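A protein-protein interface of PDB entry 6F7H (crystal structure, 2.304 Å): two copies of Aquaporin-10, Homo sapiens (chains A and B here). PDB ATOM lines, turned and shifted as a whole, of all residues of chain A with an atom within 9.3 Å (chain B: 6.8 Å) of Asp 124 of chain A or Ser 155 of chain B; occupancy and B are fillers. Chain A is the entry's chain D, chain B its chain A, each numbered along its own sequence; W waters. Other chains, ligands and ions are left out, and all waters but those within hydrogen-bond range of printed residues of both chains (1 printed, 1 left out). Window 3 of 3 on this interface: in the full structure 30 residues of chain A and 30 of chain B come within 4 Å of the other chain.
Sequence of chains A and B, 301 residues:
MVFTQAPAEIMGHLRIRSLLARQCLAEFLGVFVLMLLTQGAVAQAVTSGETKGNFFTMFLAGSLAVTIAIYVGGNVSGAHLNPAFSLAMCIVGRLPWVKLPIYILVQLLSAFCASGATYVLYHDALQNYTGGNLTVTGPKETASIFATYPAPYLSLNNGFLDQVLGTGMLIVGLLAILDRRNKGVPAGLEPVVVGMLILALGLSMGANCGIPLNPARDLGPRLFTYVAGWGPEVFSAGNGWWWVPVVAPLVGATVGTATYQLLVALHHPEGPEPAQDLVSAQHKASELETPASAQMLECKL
OD1 of Asn 158 of chain B lies within hydrogen-bond range of N of Asp 124 of chain A (2.9 Å). The side-chain hydroxyl of Ser 155 of chain B lies within hydrogen-bond range of the side-chain carboxylate of Asp 124 of chain A (2.7 Å). ND2 of Asn 208 of chain B lies within hydrogen-bond range of O of Leu 121 of chain A (3.2 Å). O of Leu 121 of chain A sits at hydrogen-bond distance from ND2 of Asn 158 of chain B (3.0 Å).
No position is printed for both chains. Of the 11 pairs that touch across the chains among the printed residues, none has its exchanged pair printed and touching as well.
Water W1 lies within hydrogen-bond range of OH of Tyr 153 of chain B (2.7 Å) and OG1 of Thr 47 of chain A (2.9 Å).
Of the printed residues of chain B, Leu 121 of chain A touches Asn 158 (3.0 Å) and Asn 208 (3.2 Å). Of the printed residues of chain B, His 123 of chain A touches Asn 158. Of chain B, only Tyr 153 (3.7 Å), Leu 154 (3.8 Å), Ser 155 (2.7 Å) and Asn 158 (2.9 Å) come within 4 Å of Asp 124 of chain A. Printed residues of chain B within 4 Å of Ala 125 of chain A: Tyr 153 (3.5 Å). Of the printed residues of chain B, Asn 128 of chain A touches Tyr 153. Of chain A, only Asp 124 comes within 4 Å of Leu 154 of chain B. Of chain A, only Asp 124 comes within 4 Å of Ser 155 of chain B. Of chain A, only Val 120 (3.7 Å), Leu 121 (3.0 Å), His 123 (3.7 Å) and Asp 124 (2.9 Å) come within 4 Å of Asn 158 of chain B. Of the printed residues of chain A, Leu 161 of chain B touches Val 120. The nearest residue of chain B that does not touch Asp 124 of chain A is Gly 159 of chain B (5.5 Å). The nearest residue of chain A that does not touch Ser 155 of chain B is His 123 of chain A (6.8 Å). The nearest printed residue of chain B that does not touch Asn 128 of chain A is Pro 152 of chain B (6.3 Å).
Of the 16 printed residues of chain A, 6 touch a printed residue of chain B. Printed residues of chain A that touch a printed residue of chain B: Val 120, Leu 121, His 123, Asp 124, Ala 125 and Asn 128. Among the printed residues, no Asp or Glu carboxylate lies within 4 Å of a Lys or Arg side-chain nitrogen of the other chain.
The side-chain hydroxyl (OH) of Tyr 153 of chain B sits at hydrogen-bond distance from the side-chain amide oxygen (OD1) of Asn 208 of chain B (2.8 Å). The side-chain carboxylate (OD1) of Asp 124 of chain A lies within hydrogen-bond range of a ring nitrogen (ND1) of His 123 of chain A, 3.2 Å away. The backbone NH of Ala 151 of chain B is in hydrogen-bond range of the backbone carbonyl oxygen of Asn 208 of chain B. OG of Ser 155 of chain B lies within hydrogen-bond range of N of Asn 158 of chain B, 3.0 Å away.
Among the printed residues, pairs that only touch across the chains: Val 120 of chain A with Asn 158 of chain B (3.7 Å), Val 120 of chain A with Leu 161 of chain B (3.7 Å), His 123 of chain A with Asn 158 of chain B (3.7 Å), Asp 124 of chain A with Tyr 153 of chain B (3.7 Å), Asp 124 of chain A with Leu 154 of chain B (3.8 Å), Ala 125 of chain A with Tyr 153 of chain B (3.5 Å) and Asn 128 of chain A with Tyr 153 of chain B (3.6 Å).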
ATOM      1  N   THR A  47       2.569  -7.475   9.070  1.00  0.00           N
ATOM      2  CA  THR A  47       2.031  -8.789   9.424  1.00  0.00           C
ATOM      3  C   THR A  47       2.933  -9.534  10.405  1.00  0.00           C
ATOM      4  O   THR A  47       2.455 -10.413  11.126  1.00  0.00           O
ATOM      5  CB  THR A  47       1.776  -9.645   8.170  1.00  0.00           C
ATOM      6  OG1 THR A  47       2.994  -9.911   7.464  1.00  0.00           O
ATOM      7  CG2 THR A  47       0.796  -8.934   7.235  1.00  0.00           C
ATOM      8  N   THR A 118       0.569  -8.766  -4.298  1.00  0.00           N
ATOM      9  CA  THR A 118       0.911  -8.607  -2.884  1.00  0.00           C
ATOM     10  C   THR A 118      -0.090  -9.338  -1.996  1.00  0.00           C
ATOM     11  O   THR A 118       0.294 -10.067  -1.065  1.00  0.00           O
ATOM     12  CB  THR A 118       0.946  -7.123  -2.511  1.00  0.00           C
ATOM     13  OG1 THR A 118       1.998  -6.469  -3.227  1.00  0.00           O
ATOM     14  CG2 THR A 118       1.143  -6.955  -1.002  1.00  0.00           C
ATOM     15  N   TYR A 119      -1.379  -9.138  -2.272  1.00  0.00           N
ATOM     16  CA  TYR A 119      -2.444  -9.739  -1.469  1.00  0.00           C
ATOM     17  C   TYR A 119      -2.343 -11.258  -1.470  1.00  0.00           C
ATOM     18  O   TYR A 119      -2.517 -11.900  -0.431  1.00  0.00           O
ATOM     19  CB  TYR A 119      -3.804  -9.270  -2.011  1.00  0.00           C
ATOM     20  CG  TYR A 119      -5.057  -9.875  -1.368  1.00  0.00           C
ATOM     21  CD1 TYR A 119      -5.562 -11.105  -1.806  1.00  0.00           C
ATOM     22  CD2 TYR A 119      -5.774  -9.191  -0.381  1.00  0.00           C
ATOM     23  CE1 TYR A 119      -6.693 -11.655  -1.243  1.00  0.00           C
ATOM     24  CE2 TYR A 119      -6.933  -9.733   0.176  1.00  0.00           C
ATOM     25  CZ  TYR A 119      -7.382 -10.972  -0.253  1.00  0.00           C
ATOM     26  OH  TYR A 119      -8.533 -11.551   0.270  1.00  0.00           O
ATOM     27  N   VAL A 120      -2.042 -11.847  -2.626  1.00  0.00           N
ATOM     28  CA  VAL A 120      -1.856 -13.293  -2.727  1.00  0.00           C
ATOM     29  C   VAL A 120      -0.541 -13.719  -2.070  1.00  0.00           C
ATOM     30  O   VAL A 120      -0.498 -14.716  -1.333  1.00  0.00           O
ATOM     31  CB  VAL A 120      -1.938 -13.726  -4.209  1.00  0.00           C
ATOM     32  CG1 VAL A 120      -1.364 -15.116  -4.386  1.00  0.00           C
ATOM     33  CG2 VAL A 120      -3.397 -13.667  -4.725  1.00  0.00           C
ATOM     34  N   LEU A 121       0.542 -12.951  -2.285  1.00  0.00           N
ATOM     35  CA  LEU A 121       1.814 -13.264  -1.615  1.00  0.00           C
ATOM     36  C   LEU A 121       1.652 -13.327  -0.093  1.00  0.00           C
ATOM     37  O   LEU A 121       2.192 -14.226   0.558  1.00  0.00           O
ATOM     38  CB  LEU A 121       2.882 -12.240  -1.994  1.00  0.00           C
ATOM     39  CG  LEU A 121       4.346 -12.481  -1.555  1.00  0.00           C
ATOM     40  CD1 LEU A 121       4.826 -13.915  -1.852  1.00  0.00           C
ATOM     41  CD2 LEU A 121       5.214 -11.480  -2.293  1.00  0.00           C
ATOM     42  N   TYR A 122       0.878 -12.415   0.489  1.00  0.00           N
ATOM     43  CA  TYR A 122       0.762 -12.325   1.944  1.00  0.00           C
ATOM     44  C   TYR A 122      -0.601 -12.778   2.473  1.00  0.00           C
ATOM     45  O   TYR A 122      -0.999 -12.365   3.568  1.00  0.00           O
ATOM     46  CB  TYR A 122       1.059 -10.894   2.386  1.00  0.00           C
ATOM     47  CG  TYR A 122       2.526 -10.625   2.419  1.00  0.00           C
ATOM     48  CD1 TYR A 122       3.205 -10.187   1.284  1.00  0.00           C
ATOM     49  CD2 TYR A 122       3.259 -10.848   3.597  1.00  0.00           C
ATOM     50  CE1 TYR A 122       4.586  -9.968   1.326  1.00  0.00           C
ATOM     51  CE2 TYR A 122       4.631 -10.609   3.661  1.00  0.00           C
ATOM     52  CZ  TYR A 122       5.285 -10.177   2.525  1.00  0.00           C
ATOM     53  OH  TYR A 122       6.633  -9.999   2.597  1.00  0.00           O
ATOM     54  N   HIS A 123      -1.314 -13.632   1.723  1.00  0.00           N
ATOM     55  CA  HIS A 123      -2.643 -14.079   2.134  1.00  0.00           C
ATOM     56  C   HIS A 123      -2.633 -14.718   3.522  1.00  0.00           C
ATOM     57  O   HIS A 123      -3.372 -14.298   4.423  1.00  0.00           O
ATOM     58  CB  HIS A 123      -3.208 -15.061   1.106  1.00  0.00           C
ATOM     59  CG  HIS A 123      -4.572 -15.546   1.454  1.00  0.00           C
ATOM     60  ND1 HIS A 123      -4.785 -16.585   2.338  1.00  0.00           N
ATOM     61  CD2 HIS A 123      -5.796 -15.108   1.071  1.00  0.00           C
ATOM     62  CE1 HIS A 123      -6.089 -16.777   2.465  1.00  0.00           C
ATOM     63  NE2 HIS A 123      -6.722 -15.899   1.705  1.00  0.00           N
ATOM     64  N   ASP A 124      -1.830 -15.769   3.701  1.00  0.00           N
ATOM     65  CA  ASP A 124      -1.773 -16.441   4.996  1.00  0.00           C
ATOM     66  C   ASP A 124      -1.333 -15.499   6.117  1.00  0.00           C
ATOM     67  O   ASP A 124      -1.869 -15.569   7.232  1.00  0.00           O
ATOM     68  CB  ASP A 124      -0.842 -17.644   4.912  1.00  0.00           C
ATOM     69  CG  ASP A 124      -1.436 -18.755   4.089  1.00  0.00           C
ATOM     70  OD1 ASP A 124      -2.544 -18.525   3.551  1.00  0.00           O
ATOM     71  OD2 ASP A 124      -0.816 -19.837   3.990  1.00  0.00           O
ATOM     72  N   ALA A 125      -0.359 -14.617   5.842  1.00  0.00           N
ATOM     73  CA  ALA A 125       0.131 -13.683   6.862  1.00  0.00           C
ATOM     74  C   ALA A 125      -0.928 -12.644   7.216  1.00  0.00           C
ATOM     75  O   ALA A 125      -1.083 -12.292   8.392  1.00  0.00           O
ATOM     76  CB  ALA A 125       1.424 -13.002   6.381  1.00  0.00           C
ATOM     77  N   LEU A 126      -1.658 -12.140   6.207  1.00  0.00           N
ATOM     78  CA  LEU A 126      -2.784 -11.228   6.431  1.00  0.00           C
ATOM     79  C   LEU A 126      -3.851 -11.866   7.307  1.00  0.00           C
ATOM     80  O   LEU A 126      -4.288 -11.282   8.308  1.00  0.00           O
ATOM     81  CB  LEU A 126      -3.411 -10.819   5.093  1.00  0.00           C
ATOM     82  CG  LEU A 126      -2.690  -9.685   4.378  1.00  0.00           C
ATOM     83  CD1 LEU A 126      -3.046  -9.708   2.896  1.00  0.00           C
ATOM     84  CD2 LEU A 126      -3.025  -8.340   5.018  1.00  0.00           C
ATOM     85  N   GLN A 127      -4.317 -13.049   6.908  1.00  0.00           N
ATOM     86  CA  GLN A 127      -5.303 -13.776   7.694  1.00  0.00           C
ATOM     87  C   GLN A 127      -4.833 -13.970   9.132  1.00  0.00           C
ATOM     88  O   GLN A 127      -5.592 -13.753  10.082  1.00  0.00           O
ATOM     89  CB  GLN A 127      -5.585 -15.128   7.038  1.00  0.00           C
ATOM     90  CG  GLN A 127      -6.705 -15.924   7.707  1.00  0.00           C
ATOM     91  CD  GLN A 127      -8.085 -15.319   7.483  1.00  0.00           C
ATOM     92  OE1 GLN A 127      -8.247 -14.344   6.741  1.00  0.00           O
ATOM     93  NE2 GLN A 127      -9.087 -15.903   8.121  1.00  0.00           N
ATOM     94  N   ASN A 128      -3.575 -14.384   9.309  1.00  0.00           N
ATOM     95  CA  ASN A 128      -3.062 -14.632  10.651  1.00  0.00           C
ATOM     96  C   ASN A 128      -2.973 -13.338  11.452  1.00  0.00           C
ATOM     97  O   ASN A 128      -3.305 -13.310  12.640  1.00  0.00           O
ATOM     98  CB  ASN A 128      -1.700 -15.319  10.557  1.00  0.00           C
ATOM     99  CG  ASN A 128      -1.080 -15.571  11.917  1.00  0.00           C
ATOM    100  OD1 ASN A 128      -1.547 -16.428  12.675  1.00  0.00           O
ATOM    101  ND2 ASN A 128      -0.020 -14.826  12.238  1.00  0.00           N
ATOM    102  N   TYR A 129      -2.552 -12.247  10.812  1.00  0.00           N
ATOM    103  CA  TYR A 129      -2.437 -10.981  11.525  1.00  0.00           C
ATOM    104  C   TYR A 129      -3.803 -10.409  11.897  1.00  0.00           C
ATOM    105  O   TYR A 129      -3.978  -9.883  13.002  1.00  0.00           O
ATOM    106  CB  TYR A 129      -1.659  -9.979  10.682  1.00  0.00           C
ATOM    107  CG  TYR A 129      -1.461  -8.621  11.345  1.00  0.00           C
ATOM    108  CD1 TYR A 129      -0.638  -8.469  12.460  1.00  0.00           C
ATOM    109  CD2 TYR A 129      -2.067  -7.488  10.819  1.00  0.00           C
ATOM    110  CE1 TYR A 129      -0.458  -7.222  13.053  1.00  0.00           C
ATOM    111  CE2 TYR A 129      -1.893  -6.245  11.392  1.00  0.00           C
ATOM    112  CZ  TYR A 129      -1.093  -6.106  12.510  1.00  0.00           C
ATOM    113  OH  TYR A 129      -0.929  -4.833  13.045  1.00  0.00           O
ATOM    114  N   THR A 130      -4.779 -10.493  10.989  1.00  0.00           N
ATOM    115  CA  THR A 130      -6.055  -9.809  11.150  1.00  0.00           C
ATOM    116  C   THR A 130      -7.186 -10.713  11.619  1.00  0.00           C
ATOM    117  O   THR A 130      -8.256 -10.200  11.962  1.00  0.00           O
ATOM    118  CB  THR A 130      -6.496  -9.183   9.822  1.00  0.00           C
ATOM    119  OG1 THR A 130      -6.878 -10.234   8.918  1.00  0.00           O
ATOM    120  CG2 THR A 130      -5.384  -8.346   9.201  1.00  0.00           C
ATOM    121  N   GLY A 131      -7.001 -12.032  11.598  1.00  0.00           N
ATOM    122  CA  GLY A 131      -8.127 -12.932  11.759  1.00  0.00           C
ATOM    123  C   GLY A 131      -9.224 -12.728  10.740  1.00  0.00           C
ATOM    124  O   GLY A 131     -10.360 -13.138  10.975  1.00  0.00           O
ATOM    125  N   GLY A 132      -8.922 -12.106   9.601  1.00  0.00           N
ATOM    126  CA  GLY A 132      -9.914 -11.841   8.581  1.00  0.00           C
ATOM    127  C   GLY A 132     -10.581 -10.484   8.669  1.00  0.00           C
ATOM    128  O   GLY A 132     -11.380 -10.150   7.795  1.00  0.00           O
ATOM    129  N   PRO B 150       9.426 -22.435   7.389  1.00  0.00           N
ATOM    130  CA  PRO B 150       8.400 -21.421   7.113  1.00  0.00           C
ATOM    131  C   PRO B 150       7.879 -20.799   8.403  1.00  0.00           C
ATOM    132  O   PRO B 150       7.940 -21.397   9.467  1.00  0.00           O
ATOM    133  CB  PRO B 150       7.284 -22.231   6.432  1.00  0.00           C
ATOM    134  CG  PRO B 150       7.354 -23.561   7.132  1.00  0.00           C
ATOM    135  CD  PRO B 150       8.883 -23.803   7.334  1.00  0.00           C
ATOM    136  N   ALA B 151       7.291 -19.608   8.276  1.00  0.00           N
ATOM    137  CA  ALA B 151       6.570 -19.024   9.397  1.00  0.00           C
ATOM    138  C   ALA B 151       5.454 -19.961   9.862  1.00  0.00           C
ATOM    139  O   ALA B 151       4.896 -20.714   9.065  1.00  0.00           O
ATOM    140  CB  ALA B 151       5.976 -17.677   9.015  1.00  0.00           C
ATOM    141  N   PRO B 152       5.104 -19.928  11.152  1.00  0.00           N
ATOM    142  CA  PRO B 152       4.063 -20.844  11.657  1.00  0.00           C
ATOM    143  C   PRO B 152       2.730 -20.748  10.939  1.00  0.00           C
ATOM    144  O   PRO B 152       2.029 -21.760  10.844  1.00  0.00           O
ATOM    145  CB  PRO B 152       3.927 -20.437  13.137  1.00  0.00           C
ATOM    146  CG  PRO B 152       5.210 -19.878  13.500  1.00  0.00           C
ATOM    147  CD  PRO B 152       5.849 -19.270  12.244  1.00  0.00           C
ATOM    148  N   TYR B 153       2.342 -19.570  10.443  1.00  0.00           N
ATOM    149  CA  TYR B 153       1.044 -19.421   9.790  1.00  0.00           C
ATOM    150  C   TYR B 153       1.038 -19.929   8.345  1.00  0.00           C
ATOM    151  O   TYR B 153      -0.031 -20.007   7.732  1.00  0.00           O
ATOM    152  CB  TYR B 153       0.623 -17.938   9.814  1.00  0.00           C
ATOM    153  CG  TYR B 153       1.617 -17.045   9.090  1.00  0.00           C
ATOM    154  CD1 TYR B 153       1.647 -17.005   7.706  1.00  0.00           C
ATOM    155  CD2 TYR B 153       2.557 -16.266   9.798  1.00  0.00           C
ATOM    156  CE1 TYR B 153       2.571 -16.208   7.019  1.00  0.00           C
ATOM    157  CE2 TYR B 153       3.501 -15.456   9.125  1.00  0.00           C
ATOM    158  CZ  TYR B 153       3.507 -15.436   7.725  1.00  0.00           C
ATOM    159  OH  TYR B 153       4.415 -14.652   7.002  1.00  0.00           O
ATOM    160  N   LEU B 154       2.187 -20.270   7.776  1.00  0.00           N
ATOM    161  CA  LEU B 154       2.301 -20.412   6.322  1.00  0.00           C
ATOM    162  C   LEU B 154       1.857 -21.798   5.846  1.00  0.00           C
ATOM    163  O   LEU B 154       2.441 -22.811   6.237  1.00  0.00           O
ATOM    164  CB  LEU B 154       3.746 -20.146   5.895  1.00  0.00           C
ATOM    165  CG  LEU B 154       3.969 -20.048   4.383  1.00  0.00           C
ATOM    166  CD1 LEU B 154       3.258 -18.804   3.815  1.00  0.00           C
ATOM    167  CD2 LEU B 154       5.441 -20.028   4.065  1.00  0.00           C
ATOM    168  N   SER B 155       0.886 -21.838   4.938  1.00  0.00           N
ATOM    169  CA  SER B 155       0.519 -23.084   4.260  1.00  0.00           C
ATOM    170  C   SER B 155       1.556 -23.458   3.191  1.00  0.00           C
ATOM    171  O   SER B 155       2.297 -22.607   2.691  1.00  0.00           O
ATOM    172  CB  SER B 155      -0.848 -22.949   3.600  1.00  0.00           C
ATOM    173  OG  SER B 155      -0.727 -22.047   2.523  1.00  0.00           O
ATOM    174  N   LEU B 156       1.602 -24.753   2.849  1.00  0.00           N
ATOM    175  CA  LEU B 156       2.434 -25.209   1.734  1.00  0.00           C
ATOM    176  C   LEU B 156       2.123 -24.449   0.440  1.00  0.00           C
ATOM    177  O   LEU B 156       3.034 -24.083  -0.310  1.00  0.00           O
ATOM    178  CB  LEU B 156       2.255 -26.715   1.511  1.00  0.00           C
ATOM    179  CG  LEU B 156       2.621 -27.646   2.681  1.00  0.00           C
ATOM    180  CD1 LEU B 156       2.334 -29.102   2.341  1.00  0.00           C
ATOM    181  CD2 LEU B 156       4.080 -27.473   3.109  1.00  0.00           C
ATOM    182  N   ASN B 157       0.838 -24.220   0.147  1.00  0.00           N
ATOM    183  CA  ASN B 157       0.493 -23.520  -1.090  1.00  0.00           C
ATOM    184  C   ASN B 157       1.044 -22.090  -1.089  1.00  0.00           C
ATOM    185  O   ASN B 157       1.607 -21.626  -2.083  1.00  0.00           O
ATOM    186  CB  ASN B 157      -1.031 -23.491  -1.295  1.00  0.00           C
ATOM    187  CG  ASN B 157      -1.652 -24.877  -1.521  1.00  0.00           C
ATOM    188  OD1 ASN B 157      -0.962 -25.890  -1.705  1.00  0.00           O
ATOM    189  ND2 ASN B 157      -2.975 -24.911  -1.522  1.00  0.00           N
ATOM    190  N   ASN B 158       0.838 -21.353   0.003  1.00  0.00           N
ATOM    191  CA  ASN B 158       1.327 -19.979   0.054  1.00  0.00           C
ATOM    192  C   ASN B 158       2.848 -19.959   0.003  1.00  0.00           C
ATOM    193  O   ASN B 158       3.443 -19.150  -0.732  1.00  0.00           O
ATOM    194  CB  ASN B 158       0.797 -19.279   1.312  1.00  0.00           C
ATOM    195  CG  ASN B 158       0.815 -17.734   1.212  1.00  0.00           C
ATOM    196  OD1 ASN B 158       0.097 -17.051   1.962  1.00  0.00           O
ATOM    197  ND2 ASN B 158       1.638 -17.184   0.305  1.00  0.00           N
ATOM    198  N   GLY B 159       3.498 -20.869   0.757  1.00  0.00           N
ATOM    199  CA  GLY B 159       4.957 -20.976   0.707  1.00  0.00           C
ATOM    200  C   GLY B 159       5.468 -21.336  -0.682  1.00  0.00           C
ATOM    201  O   GLY B 159       6.495 -20.824  -1.130  1.00  0.00           O
ATOM    202  N   PHE B 160       4.735 -22.204  -1.401  1.00  0.00           N
ATOM    203  CA  PHE B 160       5.145 -22.576  -2.752  1.00  0.00           C
ATOM    204  C   PHE B 160       5.063 -21.370  -3.682  1.00  0.00           C
ATOM    205  O   PHE B 160       5.985 -21.107  -4.468  1.00  0.00           O
ATOM    206  CB  PHE B 160       4.275 -23.734  -3.257  1.00  0.00           C
ATOM    207  CG  PHE B 160       4.762 -24.357  -4.544  1.00  0.00           C
ATOM    208  CD1 PHE B 160       4.494 -23.770  -5.753  1.00  0.00           C
ATOM    209  CD2 PHE B 160       5.484 -25.550  -4.536  1.00  0.00           C
ATOM    210  CE1 PHE B 160       4.947 -24.346  -6.939  1.00  0.00           C
ATOM    211  CE2 PHE B 160       5.945 -26.130  -5.733  1.00  0.00           C
ATOM    212  CZ  PHE B 160       5.671 -25.523  -6.924  1.00  0.00           C
ATOM    213  N   LEU B 161       4.019 -20.592  -3.528  1.00  0.00           N
ATOM    214  CA  LEU B 161       3.856 -19.415  -4.312  1.00  0.00           C
ATOM    215  C   LEU B 161       4.926 -18.373  -4.039  1.00  0.00           C
ATOM    216  O   LEU B 161       5.408 -17.746  -4.936  1.00  0.00           O
ATOM    217  CB  LEU B 161       2.486 -18.837  -4.060  1.00  0.00           C
ATOM    218  CG  LEU B 161       1.839 -18.119  -5.215  1.00  0.00           C
ATOM    219  CD1 LEU B 161       0.345 -18.312  -5.115  1.00  0.00           C
ATOM    220  CD2 LEU B 161       2.183 -16.645  -5.173  1.00  0.00           C
ATOM    221  N   ASN B 208       7.723 -14.784   4.853  1.00  0.00           N
ATOM    222  CA  ASN B 208       7.015 -16.067   4.825  1.00  0.00           C
ATOM    223  C   ASN B 208       7.963 -17.222   5.136  1.00  0.00           C
ATOM    224  O   ASN B 208       7.636 -18.126   5.925  1.00  0.00           O
ATOM    225  CB  ASN B 208       6.323 -16.296   3.459  1.00  0.00           C
ATOM    226  CG  ASN B 208       5.094 -15.415   3.259  1.00  0.00           C
ATOM    227  OD1 ASN B 208       4.351 -15.127   4.205  1.00  0.00           O
ATOM    228  ND2 ASN B 208       4.884 -14.969   2.028  1.00  0.00           N
ATOM    229  N   ASN B 239       5.165 -29.009   8.459  1.00  0.00           N
ATOM    230  CA  ASN B 239       4.302 -29.816   7.590  1.00  0.00           C
ATOM    231  C   ASN B 239       5.078 -30.391   6.406  1.00  0.00           C
ATOM    232  O   ASN B 239       4.635 -30.306   5.258  1.00  0.00           O
ATOM    233  CB  ASN B 239       3.101 -29.011   7.084  1.00  0.00           C
ATOM    234  CG  ASN B 239       2.377 -28.271   8.195  1.00  0.00           C
ATOM    235  OD1 ASN B 239       2.265 -27.037   8.153  1.00  0.00           O
ATOM    236  ND2 ASN B 239       1.873 -29.013   9.196  1.00  0.00           N
ATOM    237  N   TRP B 241       8.046 -29.371   5.246  1.00  0.00           N
ATOM    238  CA  TRP B 241       8.389 -28.211   4.448  1.00  0.00           C
ATOM    239  C   TRP B 241       9.538 -28.467   3.472  1.00  0.00           C
ATOM    240  O   TRP B 241       9.642 -27.757   2.467  1.00  0.00           O
ATOM    241  CB  TRP B 241       8.716 -27.053   5.393  1.00  0.00           C
ATOM    242  CG  TRP B 241       9.302 -25.887   4.693  1.00  0.00           C
ATOM    243  CD1 TRP B 241      10.618 -25.539   4.641  1.00  0.00           C
ATOM    244  CD2 TRP B 241       8.600 -24.923   3.908  1.00  0.00           C
ATOM    245  NE1 TRP B 241      10.778 -24.405   3.881  1.00  0.00           N
ATOM    246  CE2 TRP B 241       9.550 -24.002   3.429  1.00  0.00           C
ATOM    247  CE3 TRP B 241       7.254 -24.742   3.572  1.00  0.00           C
ATOM    248  CZ2 TRP B 241       9.199 -22.920   2.637  1.00  0.00           C
ATOM    249  CZ3 TRP B 241       6.911 -23.671   2.791  1.00  0.00           C
ATOM    250  CH2 TRP B 241       7.871 -22.778   2.325  1.00  0.00           C
ATOM    251  N   VAL B 244       9.518 -27.904  -0.540  1.00  0.00           N
ATOM    252  CA  VAL B 244       9.111 -26.648  -1.169  1.00  0.00           C
ATOM    253  C   VAL B 244      10.326 -25.827  -1.625  1.00  0.00           C
ATOM    254  O   VAL B 244      10.359 -25.407  -2.791  1.00  0.00           O
ATOM    255  CB  VAL B 244       8.184 -25.867  -0.244  1.00  0.00           C
ATOM    256  CG1 VAL B 244       7.829 -24.518  -0.864  1.00  0.00           C
ATOM    257  CG2 VAL B 244       6.944 -26.721   0.158  1.00  0.00           C
HETATM  258  O   HOH W   1       4.726 -12.178   8.156  1.00  0.00           O
